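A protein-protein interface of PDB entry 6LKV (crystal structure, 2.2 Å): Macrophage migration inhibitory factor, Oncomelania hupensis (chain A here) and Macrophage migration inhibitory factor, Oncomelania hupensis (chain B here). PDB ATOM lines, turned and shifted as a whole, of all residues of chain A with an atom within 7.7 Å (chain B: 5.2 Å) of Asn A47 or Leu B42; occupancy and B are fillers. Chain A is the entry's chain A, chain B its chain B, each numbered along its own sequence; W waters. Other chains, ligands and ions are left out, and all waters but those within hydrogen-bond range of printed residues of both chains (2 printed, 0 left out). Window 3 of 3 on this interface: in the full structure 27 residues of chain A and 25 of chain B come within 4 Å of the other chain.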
ATOM      1  N   THR A   8       8.273  -6.954 -27.990  1.00  0.00           N
ATOM      2  CA  THR A   8       7.791  -7.900 -26.958  1.00  0.00           C
ATOM      3  C   THR A   8       8.836  -8.026 -25.849  1.00  0.00           C
ATOM      4  O   THR A   8      10.043  -8.021 -26.150  1.00  0.00           O
ATOM      5  CB  THR A   8       7.457  -9.270 -27.550  1.00  0.00           C
ATOM      6  OG1 THR A   8       6.859 -10.032 -26.505  1.00  0.00           O
ATOM      7  CG2 THR A   8       8.641 -10.012 -28.129  1.00  0.00           C
ATOM      8  N   ASN A   9       8.353  -8.133 -24.616  1.00  0.00           N
ATOM      9  CA  ASN A   9       9.197  -8.404 -23.427  1.00  0.00           C
ATOM     10  C   ASN A   9       9.532  -9.900 -23.382  1.00  0.00           C
ATOM     11  O   ASN A   9      10.377 -10.262 -22.577  1.00  0.00           O
ATOM     12  CB  ASN A   9       8.543  -7.876 -22.150  1.00  0.00           C
ATOM     13  CG  ASN A   9       7.162  -8.440 -21.911  1.00  0.00           C
ATOM     14  OD1 ASN A   9       6.577  -9.105 -22.781  1.00  0.00           O
ATOM     15  ND2 ASN A   9       6.624  -8.148 -20.751  1.00  0.00           N
ATOM     16  N   ARG A  43      12.040  -7.180 -31.941  1.00  0.00           N
ATOM     17  CA  ARG A  43      12.609  -6.558 -30.734  1.00  0.00           C
ATOM     18  C   ARG A  43      12.102  -7.356 -29.531  1.00  0.00           C
ATOM     19  O   ARG A  43      11.120  -6.964 -28.911  1.00  0.00           O
ATOM     20  CB  ARG A  43      12.235  -5.088 -30.703  1.00  0.00           C
ATOM     21  CG  ARG A  43      12.562  -4.407 -32.011  1.00  0.00           C
ATOM     22  CD  ARG A  43      12.534  -2.931 -31.802  1.00  0.00           C
ATOM     23  NE  ARG A  43      12.762  -2.296 -33.092  1.00  0.00           N
ATOM     24  CZ  ARG A  43      11.996  -1.360 -33.610  1.00  0.00           C
ATOM     25  NH1 ARG A  43      10.937  -0.925 -32.932  1.00  0.00           N
ATOM     26  NH2 ARG A  43      12.335  -0.831 -34.770  1.00  0.00           N
ATOM     27  N   SER A  44      12.762  -8.470 -29.271  1.00  0.00           N
ATOM     28  CA  SER A  44      12.429  -9.382 -28.157  1.00  0.00           C
ATOM     29  C   SER A  44      13.283  -8.949 -26.974  1.00  0.00           C
ATOM     30  O   SER A  44      14.263  -8.164 -27.179  1.00  0.00           O
ATOM     31  CB  SER A  44      12.602 -10.826 -28.561  1.00  0.00           C
ATOM     32  OG  SER A  44      13.935 -11.077 -28.903  1.00  0.00           O
ATOM     33  N   GLY A  45      12.885  -9.364 -25.773  1.00  0.00           N
ATOM     34  CA  GLY A  45      13.563  -8.920 -24.538  1.00  0.00           C
ATOM     35  C   GLY A  45      13.471  -7.410 -24.388  1.00  0.00           C
ATOM     36  O   GLY A  45      14.275  -6.854 -23.650  1.00  0.00           O
ATOM     37  N   ALA A  46      12.509  -6.761 -25.060  1.00  0.00           N
ATOM     38  CA  ALA A  46      12.313  -5.306 -24.956  1.00  0.00           C
ATOM     39  C   ALA A  46      11.859  -4.962 -23.538  1.00  0.00           C
ATOM     40  O   ALA A  46      11.113  -5.739 -22.918  1.00  0.00           O
ATOM     41  CB  ALA A  46      11.298  -4.801 -25.967  1.00  0.00           C
ATOM     42  N   ASN A  47      12.258  -3.790 -23.077  1.00  0.00           N
ATOM     43  CA  ASN A  47      11.783  -3.209 -21.813  1.00  0.00           C
ATOM     44  C   ASN A  47      10.429  -2.542 -22.091  1.00  0.00           C
ATOM     45  O   ASN A  47      10.316  -1.313 -22.003  1.00  0.00           O
ATOM     46  CB  ASN A  47      12.808  -2.253 -21.222  1.00  0.00           C
ATOM     47  CG  ASN A  47      12.430  -1.882 -19.801  1.00  0.00           C
ATOM     48  OD1 ASN A  47      11.421  -2.371 -19.265  1.00  0.00           O
ATOM     49  ND2 ASN A  47      13.219  -1.002 -19.207  1.00  0.00           N
ATOM     50  N   ILE A  48       9.428  -3.350 -22.396  1.00  0.00           N
ATOM     51  CA  ILE A  48       8.064  -2.882 -22.716  1.00  0.00           C
ATOM     52  C   ILE A  48       7.129  -3.499 -21.675  1.00  0.00           C
ATOM     53  O   ILE A  48       7.167  -4.711 -21.465  1.00  0.00           O
ATOM     54  CB  ILE A  48       7.662  -3.197 -24.176  1.00  0.00           C
ATOM     55  CG1 ILE A  48       6.274  -2.620 -24.513  1.00  0.00           C
ATOM     56  CG2 ILE A  48       7.710  -4.699 -24.459  1.00  0.00           C
ATOM     57  CD1 ILE A  48       5.962  -2.570 -25.992  1.00  0.00           C
ATOM     58  N   MET A  49       6.375  -2.635 -21.016  1.00  0.00           N
ATOM     59  CA  MET A  49       5.322  -3.055 -20.073  1.00  0.00           C
ATOM     60  C   MET A  49       3.974  -2.582 -20.638  1.00  0.00           C
ATOM     61  O   MET A  49       3.919  -1.625 -21.449  1.00  0.00           O
ATOM     62  CB  MET A  49       5.579  -2.506 -18.664  1.00  0.00           C
ATOM     63  CG  MET A  49       5.544  -1.005 -18.546  1.00  0.00           C
ATOM     64  SD  MET A  49       5.310  -0.447 -16.788  1.00  0.00           S
ATOM     65  CE  MET A  49       6.721  -1.277 -16.037  1.00  0.00           C
ATOM     66  N   ARG A  54       4.397  -6.435 -16.177  1.00  0.00           N
ATOM     67  CA  ARG A  54       5.474  -7.041 -17.007  1.00  0.00           C
ATOM     68  C   ARG A  54       5.111  -8.455 -17.425  1.00  0.00           C
ATOM     69  O   ARG A  54       6.013  -9.198 -17.866  1.00  0.00           O
ATOM     70  CB  ARG A  54       6.810  -7.000 -16.261  1.00  0.00           C
ATOM     71  CG  ARG A  54       7.292  -5.586 -15.948  1.00  0.00           C
ATOM     72  CD  ARG A  54       8.780  -5.561 -15.609  1.00  0.00           C
ATOM     73  NE  ARG A  54       9.286  -4.207 -15.442  1.00  0.00           N
ATOM     74  CZ  ARG A  54       9.742  -3.424 -16.426  1.00  0.00           C
ATOM     75  NH1 ARG A  54       9.770  -3.841 -17.685  1.00  0.00           N
ATOM     76  NH2 ARG A  54      10.165  -2.201 -16.149  1.00  0.00           N
ATOM     77  N   CYS A  57       3.638  -9.349 -23.252  1.00  0.00           N
ATOM     78  CA  CYS A  57       2.827  -8.464 -24.130  1.00  0.00           C
ATOM     79  C   CYS A  57       3.518  -8.272 -25.488  1.00  0.00           C
ATOM     80  O   CYS A  57       4.719  -8.609 -25.625  1.00  0.00           O
ATOM     81  CB  CYS A  57       2.575  -7.142 -23.435  1.00  0.00           C
ATOM     82  SG  CYS A  57       4.035  -6.087 -23.210  1.00  0.00           S
ATOM     83  N   VAL B   6      10.010   5.661 -25.335  1.00  0.00           N
ATOM     84  CA  VAL B   6      11.066   6.592 -24.857  1.00  0.00           C
ATOM     85  C   VAL B   6      12.407   6.075 -25.365  1.00  0.00           C
ATOM     86  O   VAL B   6      12.777   4.966 -24.963  1.00  0.00           O
ATOM     87  CB  VAL B   6      11.030   6.727 -23.324  1.00  0.00           C
ATOM     88  CG1 VAL B   6      12.114   7.646 -22.814  1.00  0.00           C
ATOM     89  CG2 VAL B   6       9.671   7.190 -22.842  1.00  0.00           C
ATOM     90  N   THR B   8      16.262   6.905 -25.328  1.00  0.00           N
ATOM     91  CA  THR B   8      17.209   7.728 -24.530  1.00  0.00           C
ATOM     92  C   THR B   8      18.552   7.016 -24.409  1.00  0.00           C
ATOM     93  O   THR B   8      18.569   5.782 -24.230  1.00  0.00           O
ATOM     94  CB  THR B   8      16.636   8.102 -23.159  1.00  0.00           C
ATOM     95  OG1 THR B   8      17.568   9.030 -22.625  1.00  0.00           O
ATOM     96  CG2 THR B   8      16.423   6.924 -22.238  1.00  0.00           C
ATOM     97  N   GLU B  12      20.183   2.440 -18.512  1.00  0.00           N
ATOM     98  CA  GLU B  12      19.082   1.730 -17.810  1.00  0.00           C
ATOM     99  C   GLU B  12      19.307   1.748 -16.288  1.00  0.00           C
ATOM    100  O   GLU B  12      18.370   2.017 -15.561  1.00  0.00           O
ATOM    101  CB  GLU B  12      19.074   0.283 -18.311  1.00  0.00           C
ATOM    102  CG  GLU B  12      17.931  -0.553 -17.772  1.00  0.00           C
ATOM    103  CD  GLU B  12      17.926  -1.921 -18.459  1.00  0.00           C
ATOM    104  OE1 GLU B  12      17.438  -2.020 -19.622  1.00  0.00           O
ATOM    105  OE2 GLU B  12      18.520  -2.842 -17.901  1.00  0.00           O
ATOM    106  N   ILE B  15      18.103   4.731 -14.185  1.00  0.00           N
ATOM    107  CA  ILE B  15      16.677   5.142 -14.295  1.00  0.00           C
ATOM    108  C   ILE B  15      15.918   4.606 -13.090  1.00  0.00           C
ATOM    109  O   ILE B  15      16.030   3.430 -12.769  1.00  0.00           O
ATOM    110  CB  ILE B  15      16.091   4.697 -15.644  1.00  0.00           C
ATOM    111  CG1 ILE B  15      16.745   5.490 -16.777  1.00  0.00           C
ATOM    112  CG2 ILE B  15      14.571   4.851 -15.649  1.00  0.00           C
ATOM    113  CD1 ILE B  15      16.410   5.040 -18.180  1.00  0.00           C
ATOM    114  N   PHE B  19       9.937   4.262 -12.938  1.00  0.00           N
ATOM    115  CA  PHE B  19       9.804   5.330 -13.976  1.00  0.00           C
ATOM    116  C   PHE B  19       8.697   4.922 -14.944  1.00  0.00           C
ATOM    117  O   PHE B  19       7.820   5.751 -15.198  1.00  0.00           O
ATOM    118  CB  PHE B  19      11.120   5.589 -14.715  1.00  0.00           C
ATOM    119  CG  PHE B  19      10.986   6.476 -15.920  1.00  0.00           C
ATOM    120  CD1 PHE B  19      10.737   7.823 -15.753  1.00  0.00           C
ATOM    121  CD2 PHE B  19      11.074   5.980 -17.208  1.00  0.00           C
ATOM    122  CE1 PHE B  19      10.555   8.654 -16.850  1.00  0.00           C
ATOM    123  CE2 PHE B  19      10.879   6.807 -18.302  1.00  0.00           C
ATOM    124  CZ  PHE B  19      10.633   8.153 -18.124  1.00  0.00           C
ATOM    125  N   GLN B  20       8.712   3.685 -15.446  1.00  0.00           N
ATOM    126  CA  GLN B  20       7.714   3.231 -16.443  1.00  0.00           C
ATOM    127  C   GLN B  20       6.315   3.212 -15.821  1.00  0.00           C
ATOM    128  O   GLN B  20       5.358   3.670 -16.503  1.00  0.00           O
ATOM    129  CB  GLN B  20       8.119   1.872 -17.003  1.00  0.00           C
ATOM    130  CG  GLN B  20       9.212   1.978 -18.040  1.00  0.00           C
ATOM    131  CD  GLN B  20       9.765   0.617 -18.341  1.00  0.00           C
ATOM    132  OE1 GLN B  20      10.602   0.140 -17.592  1.00  0.00           O
ATOM    133  NE2 GLN B  20       9.309  -0.001 -19.422  1.00  0.00           N
ATOM    134  N   VAL B  40       4.246   1.263 -22.134  1.00  0.00           N
ATOM    135  CA  VAL B  40       5.472   2.105 -22.087  1.00  0.00           C
ATOM    136  C   VAL B  40       6.666   1.239 -22.504  1.00  0.00           C
ATOM    137  O   VAL B  40       6.974   0.212 -21.822  1.00  0.00           O
ATOM    138  CB  VAL B  40       5.675   2.761 -20.717  1.00  0.00           C
ATOM    139  CG1 VAL B  40       6.917   3.632 -20.719  1.00  0.00           C
ATOM    140  CG2 VAL B  40       4.460   3.567 -20.315  1.00  0.00           C
ATOM    141  N   ASP B  41       7.277   1.637 -23.608  1.00  0.00           N
ATOM    142  CA  ASP B  41       8.432   0.944 -24.232  1.00  0.00           C
ATOM    143  C   ASP B  41       9.643   1.823 -23.984  1.00  0.00           C
ATOM    144  O   ASP B  41       9.756   2.858 -24.641  1.00  0.00           O
ATOM    145  CB  ASP B  41       8.185   0.699 -25.712  1.00  0.00           C
ATOM    146  CG  ASP B  41       9.234  -0.150 -26.399  1.00  0.00           C
ATOM    147  OD1 ASP B  41      10.243  -0.526 -25.741  1.00  0.00           O
ATOM    148  OD2 ASP B  41       8.962  -0.478 -27.574  1.00  0.00           O
ATOM    149  N   LEU B  42      10.473   1.440 -23.010  1.00  0.00           N
ATOM    150  CA  LEU B  42      11.683   2.213 -22.634  1.00  0.00           C
ATOM    151  C   LEU B  42      12.877   1.620 -23.378  1.00  0.00           C
ATOM    152  O   LEU B  42      13.269   0.475 -23.082  1.00  0.00           O
ATOM    153  CB  LEU B  42      11.844   2.187 -21.110  1.00  0.00           C
ATOM    154  CG  LEU B  42      13.097   2.901 -20.601  1.00  0.00           C
ATOM    155  CD1 LEU B  42      13.167   4.348 -21.046  1.00  0.00           C
ATOM    156  CD2 LEU B  42      13.158   2.828 -19.085  1.00  0.00           C
ATOM    157  N   ARG B  43      13.417   2.368 -24.325  1.00  0.00           N
ATOM    158  CA  ARG B  43      14.696   2.048 -24.985  1.00  0.00           C
ATOM    159  C   ARG B  43      15.773   2.908 -24.335  1.00  0.00           C
ATOM    160  O   ARG B  43      16.099   3.960 -24.879  1.00  0.00           O
ATOM    161  CB  ARG B  43      14.538   2.243 -26.491  1.00  0.00           C
ATOM    162  CG  ARG B  43      13.527   1.271 -27.053  1.00  0.00           C
ATOM    163  CD  ARG B  43      12.334   1.972 -27.590  1.00  0.00           C
ATOM    164  NE  ARG B  43      11.479   1.136 -28.400  1.00  0.00           N
ATOM    165  CZ  ARG B  43      11.226   1.319 -29.692  1.00  0.00           C
ATOM    166  NH1 ARG B  43      11.716   2.367 -30.344  1.00  0.00           N
ATOM    167  NH2 ARG B  43      10.338   0.532 -30.268  1.00  0.00           N
ATOM    168  N   SER B  44      16.279   2.465 -23.199  1.00  0.00           N
ATOM    169  CA  SER B  44      17.369   3.141 -22.461  1.00  0.00           C
ATOM    170  C   SER B  44      18.690   2.574 -22.960  1.00  0.00           C
ATOM    171  O   SER B  44      18.671   1.525 -23.642  1.00  0.00           O
ATOM    172  CB  SER B  44      17.168   2.989 -20.950  1.00  0.00           C
ATOM    173  OG  SER B  44      17.317   1.654 -20.537  1.00  0.00           O
HETATM  174  O   HOH W   1      12.620  -1.598 -25.008  1.00  0.00           O
HETATM  175  O   HOH W   2      15.523  -0.143 -20.500  1.00  0.00           O
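Hydrophobic or aromatic side chains of chain B within 4 Å of the printed part of chain A: Leu B42.
Along chain B the printed residues that touch a printed residue of chain A span positions 20 to 43.
Of the 11 printed residues of chain A, 5 touch a printed residue of chain B.
Printed residues of chain A that touch a printed residue of chain B: Arg A43, Asn A47, Ile A48, Met A49 and Arg A54.
Hydrophobic or aromatic side chains of chain A within 4 Å of the printed part of chain B: Ile A48 and Met A49.
Among the printed residues, no Asp or Glu carboxylate lies within 4 Å of a Lys or Arg side-chain nitrogen of the other chain.
Water W2 lies within hydrogen-bond range of the side-chain hydroxyl of Ser B44, the side-chain amide nitrogen of Asn A47, the side-chain carboxylate of Glu B12 and the backbone carbonyl oxygen of Leu B42.
Water W1 lies within hydrogen-bond range of the side-chain carboxylate of Asp B41 (2.7 Å), the backbone carbonyl oxygen of Leu B42 (2.9 Å) and the backbone NH of Asn A47 (2.9 Å).
The side-chain amide nitrogen (ND2) of Asn A9 sits at hydrogen-bond distance from the backbone carbonyl oxygen (O) of Arg A54, at 3.1 Å.
O of Arg A43 sits at hydrogen-bond distance from N of Thr A8 (3.0 Å).
N of Val B6 sits at hydrogen-bond distance from O of Asp B41 (2.9 Å).
The side-chain amide nitrogen (NE2) of Gln B20 is in hydrogen-bond range of the backbone carbonyl oxygen (O) of Val B40 (3.4 Å).
The backbone carbonyl oxygen (O) of Arg B43 lies within hydrogen-bond range of the backbone NH (N) of Thr B8, at 3.0 Å.
The backbone NH (N) of Arg B43 sits at hydrogen-bond distance from the backbone carbonyl oxygen (O) of Val B6, at 2.8 Å.
Asn A47 touches Val B40.
Asp B41 touches Asn A47.
O of Val B40 touches CA of Ile A48 (3.4 Å).
CD1 of Ile A48 touches CB of Asp B41, at 3.96 Å.
Met A49 touches Gln B20.
N of Val B40 lies within hydrogen-bond range of O of Met A49 (3.0 Å).
O of Asn A47 sits at hydrogen-bond distance from N of Leu B42 (2.9 Å).
NE2 of Gln B20 lies within hydrogen-bond range of O of Asn A47, 3.1 Å away.
The guanidinium group of Arg A54 lies within hydrogen-bond range of the side-chain amide oxygen of Gln B20, 2.8 Å away.
The guanidinium group (NH2) of Arg B43 sits close to the guanidinium group (NH1) of Arg A43.
Of the printed residues of chain B, Arg A43 touches Arg B43 (3.1 Å).
Of the printed residues of chain B, Asn A47 touches Gln B20, Val B40, Asp B41 and Leu B42.
Cys A57 touches none of the printed residues of chain B.
Of chain A, only Asn A47 (2.9 Å) comes within 4 Å of Leu B42.
Printed residues of chain A within 4 Å of Arg B43: Arg A43 (3.1 Å).
The nearest printed residue of chain B that does not touch Met A49 is Asp B41 (5.1 Å).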
